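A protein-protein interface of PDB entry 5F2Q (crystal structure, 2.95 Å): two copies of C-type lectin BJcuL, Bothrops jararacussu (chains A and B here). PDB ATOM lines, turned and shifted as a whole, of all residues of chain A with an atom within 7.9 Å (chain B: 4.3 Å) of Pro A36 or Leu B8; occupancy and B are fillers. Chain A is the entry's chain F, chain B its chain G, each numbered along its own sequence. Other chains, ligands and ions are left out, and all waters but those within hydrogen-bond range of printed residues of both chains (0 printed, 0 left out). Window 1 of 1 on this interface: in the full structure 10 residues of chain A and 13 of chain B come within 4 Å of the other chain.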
ATOM      1  N   CYS A  31      -5.848  -4.885  15.481  1.00  0.00           N
ATOM      2  CA  CYS A  31      -5.920  -3.941  16.593  1.00  0.00           C
ATOM      3  C   CYS A  31      -6.251  -4.666  17.893  1.00  0.00           C
ATOM      4  O   CYS A  31      -5.534  -4.541  18.893  1.00  0.00           O
ATOM      5  CB  CYS A  31      -6.969  -2.856  16.314  1.00  0.00           C
ATOM      6  SG  CYS A  31      -6.719  -1.812  14.837  1.00  0.00           S
ATOM      7  N   ARG A  32      -7.337  -5.446  17.885  1.00  0.00           N
ATOM      8  CA  ARG A  32      -7.823  -6.103  19.095  1.00  0.00           C
ATOM      9  C   ARG A  32      -6.714  -6.856  19.816  1.00  0.00           C
ATOM     10  O   ARG A  32      -6.582  -6.766  21.042  1.00  0.00           O
ATOM     11  CB  ARG A  32      -8.959  -7.057  18.739  1.00  0.00           C
ATOM     12  CG  ARG A  32     -10.184  -6.362  18.190  1.00  0.00           C
ATOM     13  CD  ARG A  32     -11.309  -6.360  19.202  1.00  0.00           C
ATOM     14  NE  ARG A  32     -11.886  -7.691  19.357  1.00  0.00           N
ATOM     15  CZ  ARG A  32     -12.832  -8.200  18.570  1.00  0.00           C
ATOM     16  NH1 ARG A  32     -13.290  -9.425  18.798  1.00  0.00           N
ATOM     17  NH2 ARG A  32     -13.322  -7.494  17.558  1.00  0.00           N
ATOM     18  N   LYS A  33      -5.911  -7.616  19.074  1.00  0.00           N
ATOM     19  CA  LYS A  33      -4.879  -8.443  19.683  1.00  0.00           C
ATOM     20  C   LYS A  33      -3.539  -7.734  19.820  1.00  0.00           C
ATOM     21  O   LYS A  33      -2.652  -8.256  20.505  1.00  0.00           O
ATOM     22  CB  LYS A  33      -4.704  -9.735  18.878  1.00  0.00           C
ATOM     23  CG  LYS A  33      -5.903 -10.674  18.972  1.00  0.00           C
ATOM     24  CD  LYS A  33      -6.011 -11.342  20.344  1.00  0.00           C
ATOM     25  CE  LYS A  33      -4.943 -12.420  20.537  1.00  0.00           C
ATOM     26  NZ  LYS A  33      -4.975 -13.027  21.898  1.00  0.00           N
ATOM     27  N   TYR A  34      -3.361  -6.564  19.200  1.00  0.00           N
ATOM     28  CA  TYR A  34      -2.170  -5.772  19.484  1.00  0.00           C
ATOM     29  C   TYR A  34      -2.025  -5.552  20.979  1.00  0.00           C
ATOM     30  O   TYR A  34      -0.924  -5.659  21.531  1.00  0.00           O
ATOM     31  CB  TYR A  34      -2.232  -4.420  18.767  1.00  0.00           C
ATOM     32  CG  TYR A  34      -0.999  -3.561  18.990  1.00  0.00           C
ATOM     33  CD1 TYR A  34       0.007  -3.495  18.036  1.00  0.00           C
ATOM     34  CD2 TYR A  34      -0.837  -2.826  20.160  1.00  0.00           C
ATOM     35  CE1 TYR A  34       1.137  -2.721  18.237  1.00  0.00           C
ATOM     36  CE2 TYR A  34       0.290  -2.051  20.372  1.00  0.00           C
ATOM     37  CZ  TYR A  34       1.274  -2.001  19.407  1.00  0.00           C
ATOM     38  OH  TYR A  34       2.398  -1.229  19.605  1.00  0.00           O
ATOM     39  N   LYS A  35      -3.134  -5.249  21.650  1.00  0.00           N
ATOM     40  CA  LYS A  35      -3.128  -4.935  23.070  1.00  0.00           C
ATOM     41  C   LYS A  35      -4.564  -4.998  23.564  1.00  0.00           C
ATOM     42  O   LYS A  35      -5.490  -4.737  22.789  1.00  0.00           O
ATOM     43  CB  LYS A  35      -2.527  -3.543  23.326  1.00  0.00           C
ATOM     44  CG  LYS A  35      -2.491  -3.127  24.781  1.00  0.00           C
ATOM     45  CD  LYS A  35      -2.332  -1.628  24.930  1.00  0.00           C
ATOM     46  CE  LYS A  35      -2.446  -1.217  26.388  1.00  0.00           C
ATOM     47  NZ  LYS A  35      -3.677  -1.741  27.055  1.00  0.00           N
ATOM     48  N   PRO A  36      -4.790  -5.369  24.823  1.00  0.00           N
ATOM     49  CA  PRO A  36      -6.159  -5.345  25.352  1.00  0.00           C
ATOM     50  C   PRO A  36      -6.749  -3.942  25.321  1.00  0.00           C
ATOM     51  O   PRO A  36      -6.104  -2.968  25.714  1.00  0.00           O
ATOM     52  CB  PRO A  36      -5.993  -5.854  26.786  1.00  0.00           C
ATOM     53  CG  PRO A  36      -4.738  -6.629  26.773  1.00  0.00           C
ATOM     54  CD  PRO A  36      -3.842  -5.955  25.785  1.00  0.00           C
ATOM     55  N   GLY A  37      -7.991  -3.852  24.857  1.00  0.00           N
ATOM     56  CA  GLY A  37      -8.684  -2.580  24.790  1.00  0.00           C
ATOM     57  C   GLY A  37      -8.393  -1.782  23.540  1.00  0.00           C
ATOM     58  O   GLY A  37      -8.236  -0.557  23.612  1.00  0.00           O
ATOM     59  N   CYS A  38      -8.315  -2.441  22.388  1.00  0.00           N
ATOM     60  CA  CYS A  38      -8.068  -1.768  21.122  1.00  0.00           C
ATOM     61  C   CYS A  38      -9.168  -2.109  20.126  1.00  0.00           C
ATOM     62  O   CYS A  38      -9.764  -3.188  20.174  1.00  0.00           O
ATOM     63  CB  CYS A  38      -6.710  -2.161  20.530  1.00  0.00           C
ATOM     64  SG  CYS A  38      -5.249  -1.672  21.492  1.00  0.00           S
ATOM     65  N   HIS A  39      -9.428  -1.170  19.220  1.00  0.00           N
ATOM     66  CA  HIS A  39     -10.371  -1.376  18.132  1.00  0.00           C
ATOM     67  C   HIS A  39      -9.941  -0.504  16.963  1.00  0.00           C
ATOM     68  O   HIS A  39      -9.013   0.302  17.068  1.00  0.00           O
ATOM     69  CB  HIS A  39     -11.809  -1.024  18.538  1.00  0.00           C
ATOM     70  CG  HIS A  39     -12.366  -1.879  19.633  1.00  0.00           C
ATOM     71  ND1 HIS A  39     -12.121  -1.636  20.967  1.00  0.00           N
ATOM     72  CD2 HIS A  39     -13.174  -2.965  19.592  1.00  0.00           C
ATOM     73  CE1 HIS A  39     -12.745  -2.541  21.700  1.00  0.00           C
ATOM     74  NE2 HIS A  39     -13.392  -3.359  20.890  1.00  0.00           N
ATOM     75  N   GLN A 132      -7.204   2.174  17.605  1.00  0.00           N
ATOM     76  CA  GLN A 132      -7.561   3.023  18.732  1.00  0.00           C
ATOM     77  C   GLN A 132      -7.401   2.188  19.991  1.00  0.00           C
ATOM     78  O   GLN A 132      -7.946   1.084  20.064  1.00  0.00           O
ATOM     79  CB  GLN A 132      -8.999   3.525  18.581  1.00  0.00           C
ATOM     80  CG  GLN A 132      -9.540   4.356  19.718  1.00  0.00           C
ATOM     81  CD  GLN A 132     -11.023   4.600  19.554  1.00  0.00           C
ATOM     82  OE1 GLN A 132     -11.453   5.708  19.230  1.00  0.00           O
ATOM     83  NE2 GLN A 132     -11.818   3.555  19.762  1.00  0.00           N
ATOM     84  N   CYS A 133      -6.648   2.694  20.967  1.00  0.00           N
ATOM     85  CA  CYS A 133      -6.292   1.896  22.132  1.00  0.00           C
ATOM     86  C   CYS A 133      -6.356   2.726  23.404  1.00  0.00           C
ATOM     87  O   CYS A 133      -6.036   3.918  23.410  1.00  0.00           O
ATOM     88  CB  CYS A 133      -4.881   1.306  22.006  1.00  0.00           C
ATOM     89  SG  CYS A 133      -4.658   0.099  20.680  1.00  0.00           S
ATOM     90  N   LYS A 134      -6.777   2.073  24.484  1.00  0.00           N
ATOM     91  CA  LYS A 134      -6.572   2.589  25.825  1.00  0.00           C
ATOM     92  C   LYS A 134      -5.174   2.210  26.311  1.00  0.00           C
ATOM     93  O   LYS A 134      -4.566   1.249  25.836  1.00  0.00           O
ATOM     94  CB  LYS A 134      -7.622   2.026  26.788  1.00  0.00           C
ATOM     95  CG  LYS A 134      -9.087   2.191  26.374  1.00  0.00           C
ATOM     96  CD  LYS A 134      -9.991   1.401  27.335  1.00  0.00           C
ATOM     97  CE  LYS A 134     -11.461   1.406  26.923  1.00  0.00           C
ATOM     98  NZ  LYS A 134     -12.302   0.533  27.811  1.00  0.00           N
ATOM     99  N   PHE A 135      -4.664   2.979  27.272  1.00  0.00           N
ATOM    100  CA  PHE A 135      -3.375   2.662  27.893  1.00  0.00           C
ATOM    101  C   PHE A 135      -3.350   2.993  29.388  1.00  0.00           C
ATOM    102  O   PHE A 135      -2.384   2.667  30.084  1.00  0.00           O
ATOM    103  CB  PHE A 135      -2.237   3.406  27.187  1.00  0.00           C
ATOM    104  CG  PHE A 135      -1.767   2.746  25.917  1.00  0.00           C
ATOM    105  CD1 PHE A 135      -2.322   3.083  24.695  1.00  0.00           C
ATOM    106  CD2 PHE A 135      -0.758   1.798  25.947  1.00  0.00           C
ATOM    107  CE1 PHE A 135      -1.884   2.480  23.522  1.00  0.00           C
ATOM    108  CE2 PHE A 135      -0.318   1.193  24.780  1.00  0.00           C
ATOM    109  CZ  PHE A 135      -0.881   1.536  23.567  1.00  0.00           C
ATOM    110  OXT PHE A 135      -4.281   3.590  29.937  1.00  0.00           O
ATOM    111  N   GLN B   5       0.687  -3.297  29.803  1.00  0.00           N
ATOM    112  CA  GLN B   5       0.145  -3.481  28.462  1.00  0.00           C
ATOM    113  C   GLN B   5      -0.601  -4.799  28.308  1.00  0.00           C
ATOM    114  O   GLN B   5      -1.569  -4.861  27.544  1.00  0.00           O
ATOM    115  CB  GLN B   5       1.255  -3.378  27.417  1.00  0.00           C
ATOM    116  CG  GLN B   5       1.670  -1.940  27.134  1.00  0.00           C
ATOM    117  CD  GLN B   5       2.347  -1.768  25.788  1.00  0.00           C
ATOM    118  OE1 GLN B   5       2.205  -2.606  24.892  1.00  0.00           O
ATOM    119  NE2 GLN B   5       3.085  -0.672  25.636  1.00  0.00           N
ATOM    120  N   ASP B   6      -0.184  -5.852  29.010  1.00  0.00           N
ATOM    121  CA  ASP B   6      -0.933  -7.103  28.949  1.00  0.00           C
ATOM    122  C   ASP B   6      -2.245  -7.045  29.724  1.00  0.00           C
ATOM    123  O   ASP B   6      -2.981  -8.037  29.730  1.00  0.00           O
ATOM    124  CB  ASP B   6      -0.074  -8.257  29.471  1.00  0.00           C
ATOM    125  CG  ASP B   6       0.502  -7.982  30.843  1.00  0.00           C
ATOM    126  OD1 ASP B   6       0.816  -6.807  31.124  1.00  0.00           O
ATOM    127  OD2 ASP B   6       0.642  -8.936  31.640  1.00  0.00           O
ATOM    128  N   TRP B   7      -2.557  -5.920  30.360  1.00  0.00           N
ATOM    129  CA  TRP B   7      -3.767  -5.756  31.150  1.00  0.00           C
ATOM    130  C   TRP B   7      -4.775  -4.871  30.425  1.00  0.00           C
ATOM    131  O   TRP B   7      -4.423  -4.063  29.561  1.00  0.00           O
ATOM    132  CB  TRP B   7      -3.436  -5.152  32.517  1.00  0.00           C
ATOM    133  CG  TRP B   7      -2.735  -6.102  33.425  1.00  0.00           C
ATOM    134  CD1 TRP B   7      -1.496  -6.636  33.251  1.00  0.00           C
ATOM    135  CD2 TRP B   7      -3.231  -6.631  34.656  1.00  0.00           C
ATOM    136  NE1 TRP B   7      -1.188  -7.469  34.297  1.00  0.00           N
ATOM    137  CE2 TRP B   7      -2.239  -7.483  35.175  1.00  0.00           C
ATOM    138  CE3 TRP B   7      -4.421  -6.468  35.369  1.00  0.00           C
ATOM    139  CZ2 TRP B   7      -2.398  -8.171  36.376  1.00  0.00           C
ATOM    140  CZ3 TRP B   7      -4.578  -7.150  36.559  1.00  0.00           C
ATOM    141  CH2 TRP B   7      -3.573  -7.991  37.051  1.00  0.00           C
ATOM    142  N   LEU B   8      -6.048  -5.021  30.803  1.00  0.00           N
ATOM    143  CA  LEU B   8      -7.132  -4.259  30.195  1.00  0.00           C
ATOM    144  C   LEU B   8      -7.490  -3.071  31.072  1.00  0.00           C
ATOM    145  O   LEU B   8      -7.943  -3.275  32.208  1.00  0.00           O
ATOM    146  CB  LEU B   8      -8.363  -5.133  29.998  1.00  0.00           C
ATOM    147  CG  LEU B   8      -9.589  -4.376  29.470  1.00  0.00           C
ATOM    148  CD1 LEU B   8      -9.366  -3.946  28.028  1.00  0.00           C
ATOM    149  CD2 LEU B   8     -10.853  -5.211  29.604  1.00  0.00           C
ATOM    150  N   PRO B   9      -7.335  -1.834  30.605  1.00  0.00           N
ATOM    151  CA  PRO B   9      -7.792  -0.680  31.395  1.00  0.00           C
ATOM    152  C   PRO B   9      -9.291  -0.455  31.233  1.00  0.00           C
ATOM    153  O   PRO B   9      -9.820  -0.479  30.119  1.00  0.00           O
ATOM    154  CB  PRO B   9      -6.986   0.486  30.814  1.00  0.00           C
ATOM    155  CG  PRO B   9      -6.700   0.065  29.420  1.00  0.00           C
ATOM    156  CD  PRO B   9      -6.511  -1.421  29.457  1.00  0.00           C
ATOM    157  N   MET B  10      -9.974  -0.229  32.356  1.00  0.00           N
ATOM    158  CA  MET B  10     -11.413   0.031  32.335  1.00  0.00           C
ATOM    159  C   MET B  10     -11.799   0.777  33.603  1.00  0.00           C
ATOM    160  O   MET B  10     -11.559   0.280  34.709  1.00  0.00           O
ATOM    161  CB  MET B  10     -12.202  -1.271  32.214  1.00  0.00           C
ATOM    162  CG  MET B  10     -13.673  -1.068  31.894  1.00  0.00           C
ATOM    163  SD  MET B  10     -14.595  -2.611  31.761  1.00  0.00           S
ATOM    164  CE  MET B  10     -14.624  -3.131  33.476  1.00  0.00           C
ATOM    165  N   LEU B  13      -9.424   1.022  36.741  1.00  0.00           N
ATOM    166  CA  LEU B  13      -8.749  -0.174  37.219  1.00  0.00           C
ATOM    167  C   LEU B  13      -8.195  -0.957  36.036  1.00  0.00           C
ATOM    168  O   LEU B  13      -8.464  -0.652  34.871  1.00  0.00           O
ATOM    169  CB  LEU B  13      -9.697  -1.054  38.045  1.00  0.00           C
ATOM    170  CG  LEU B  13     -10.155  -0.505  39.397  1.00  0.00           C
ATOM    171  CD1 LEU B  13     -11.176  -1.448  40.019  1.00  0.00           C
ATOM    172  CD2 LEU B  13      -8.974  -0.299  40.337  1.00  0.00           C
ATOM    173  N   CYS B  14      -7.402  -1.974  36.355  1.00  0.00           N
ATOM    174  CA  CYS B  14      -6.770  -2.830  35.365  1.00  0.00           C
ATOM    175  C   CYS B  14      -7.248  -4.260  35.562  1.00  0.00           C
ATOM    176  O   CYS B  14      -7.311  -4.754  36.692  1.00  0.00           O
ATOM    177  CB  CYS B  14      -5.240  -2.758  35.474  1.00  0.00           C
ATOM    178  SG  CYS B  14      -4.583  -1.071  35.537  1.00  0.00           S
ATOM    179  N   TYR B  15      -7.583  -4.920  34.457  1.00  0.00           N
ATOM    180  CA  TYR B  15      -8.094  -6.280  34.464  1.00  0.00           C
ATOM    181  C   TYR B  15      -7.223  -7.155  33.576  1.00  0.00           C
ATOM    182  O   TYR B  15      -6.665  -6.688  32.581  1.00  0.00           O
ATOM    183  CB  TYR B  15      -9.544  -6.326  33.966  1.00  0.00           C
ATOM    184  CG  TYR B  15     -10.524  -5.554  34.825  1.00  0.00           C
ATOM    185  CD1 TYR B  15     -10.625  -4.170  34.732  1.00  0.00           C
ATOM    186  CD2 TYR B  15     -11.357  -6.210  35.718  1.00  0.00           C
ATOM    187  CE1 TYR B  15     -11.522  -3.463  35.513  1.00  0.00           C
ATOM    188  CE2 TYR B  15     -12.255  -5.512  36.501  1.00  0.00           C
ATOM    189  CZ  TYR B  15     -12.333  -4.140  36.393  1.00  0.00           C
ATOM    190  OH  TYR B  15     -13.226  -3.439  37.167  1.00  0.00           O
ATOM    191  N   ILE B  52     -15.762  -6.487  29.162  1.00  0.00           N
ATOM    192  CA  ILE B  52     -15.064  -7.665  29.667  1.00  0.00           C
ATOM    193  C   ILE B  52     -15.315  -8.860  28.757  1.00  0.00           C
ATOM    194  O   ILE B  52     -14.397  -9.626  28.442  1.00  0.00           O
ATOM    195  CB  ILE B  52     -15.506  -7.949  31.118  1.00  0.00           C
ATOM    196  CG1 ILE B  52     -15.172  -6.763  32.031  1.00  0.00           C
ATOM    197  CG2 ILE B  52     -14.876  -9.234  31.653  1.00  0.00           C
ATOM    198  CD1 ILE B  52     -13.689  -6.453  32.153  1.00  0.00           C
ATOM    199  N   TYR B  55     -13.050  -8.750  25.740  1.00  0.00           N
ATOM    200  CA  TYR B  55     -11.653  -8.942  26.118  1.00  0.00           C
ATOM    201  C   TYR B  55     -11.337 -10.421  26.303  1.00  0.00           C
ATOM    202  O   TYR B  55     -10.392 -10.949  25.708  1.00  0.00           O
ATOM    203  CB  TYR B  55     -11.340  -8.166  27.397  1.00  0.00           C
ATOM    204  CG  TYR B  55     -10.037  -8.574  28.048  1.00  0.00           C
ATOM    205  CD1 TYR B  55      -8.839  -8.497  27.353  1.00  0.00           C
ATOM    206  CD2 TYR B  55     -10.003  -9.033  29.358  1.00  0.00           C
ATOM    207  CE1 TYR B  55      -7.645  -8.869  27.943  1.00  0.00           C
ATOM    208  CE2 TYR B  55      -8.811  -9.406  29.957  1.00  0.00           C
ATOM    209  CZ  TYR B  55      -7.638  -9.321  29.244  1.00  0.00           C
ATOM    210  OH  TYR B  55      -6.452  -9.689  29.830  1.00  0.00           O
ATOM    211  N   TYR B  59      -8.739 -12.990  24.318  1.00  0.00           N
ATOM    212  CA  TYR B  59      -7.512 -13.338  25.025  1.00  0.00           C
ATOM    213  C   TYR B  59      -7.627 -14.591  25.881  1.00  0.00           C
ATOM    214  O   TYR B  59      -6.668 -14.931  26.584  1.00  0.00           O
ATOM    215  CB  TYR B  59      -7.070 -12.163  25.903  1.00  0.00           C
ATOM    216  CG  TYR B  59      -6.462 -11.028  25.117  1.00  0.00           C
ATOM    217  CD1 TYR B  59      -7.262 -10.058  24.531  1.00  0.00           C
ATOM    218  CD2 TYR B  59      -5.087 -10.930  24.957  1.00  0.00           C
ATOM    219  CE1 TYR B  59      -6.709  -9.022  23.812  1.00  0.00           C
ATOM    220  CE2 TYR B  59      -4.526  -9.898  24.241  1.00  0.00           C
ATOM    221  CZ  TYR B  59      -5.339  -8.946  23.670  1.00  0.00           C
ATOM    222  OH  TYR B  59      -4.773  -7.917  22.955  1.00  0.00           O
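No position is printed for both chains.
The backbone carbonyl oxygen (O) of Lys A134 lies close to the side-chain amino group (NZ) of Lys A35, at 3.3 Å. N of Lys A134 is in hydrogen-bond range of O of Gly A37 (3.1 Å). The backbone NH (N) of Leu B8 is in hydrogen-bond range of the backbone carbonyl oxygen (O) of Tyr B15. SG of Cys A38 forms a disulfide with SG of Cys A133 (2.0 Å).
The side-chain hydroxyl of Tyr B59 lies within hydrogen-bond range of the backbone carbonyl oxygen of Arg A32 (2.9 Å). The backbone carbonyl oxygen of Lys A33 sits at hydrogen-bond distance from the side-chain hydroxyl of Tyr B59. NZ of Lys A35 lies within hydrogen-bond range of O of Trp B7 (3.5 Å). The side-chain hydroxyl (OH) of Tyr B59 lies close to the backbone carbonyl oxygen (O) of Lys A35 (3.3 Å). The backbone nitrogen (N) of Pro A36 lies close to the side-chain hydroxyl (OH) of Tyr B59, at 3.2 Å.
Along chain B the printed residues that touch a printed residue of chain A span positions 5 to 59. Printed residues of chain A that touch a printed residue of chain B: Arg A32, Lys A33, Lys A35, Pro A36, Gly A37, Lys A134 and Phe A135. Among the printed residues, 15 pairs touch across the chains. Among the printed residues, no Asp or Glu carboxylate lies within 4 Å of a Lys or Arg side-chain nitrogen of the other chain.
Among the printed residues, pairs that only touch across the chains: Pro A36 with Gln B5 (3.1 Å), Lys A134 with Pro B9 (3.4 Å), Lys A35 with Gln B5 (3.4 Å), Gly A37 with Leu B8 (3.5 Å), Pro A36 with Tyr B55 (3.6 Å), Pro A36 with Trp B7 (3.7 Å), Pro A36 with Asp B6 (3.7 Å), Lys A35 with Pro B9 (3.7 Å), Pro A36 with Leu B8 (3.8 Å) and Phe A135 with Gln B5 (3.97 Å).
Printed residues of chain B within 4 Å of Pro A36: Gln B5 (3.1 Å), Asp B6 (3.7 Å), Trp B7 (3.7 Å), Leu B8 (3.8 Å), Tyr B55 (3.6 Å) and Tyr B59 (3.2 Å). Of chain A, only Pro A36 (3.8 Å) and Gly A37 (3.5 Å) come within 4 Å of Leu B8. Pro B9 touches two residues of chain A. Printed residues of chain B within 4 Å of Arg A32: Tyr B59. Of the printed residues of chain A, Tyr B55 touches Pro A36 (3.6 Å). Gln A132 touches none of the printed residues of chain B. Tyr A34 touches none of the printed residues of chain B. The nearest residue of chain B that does not touch Pro A36 is Pro B9 (4.1 Å).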
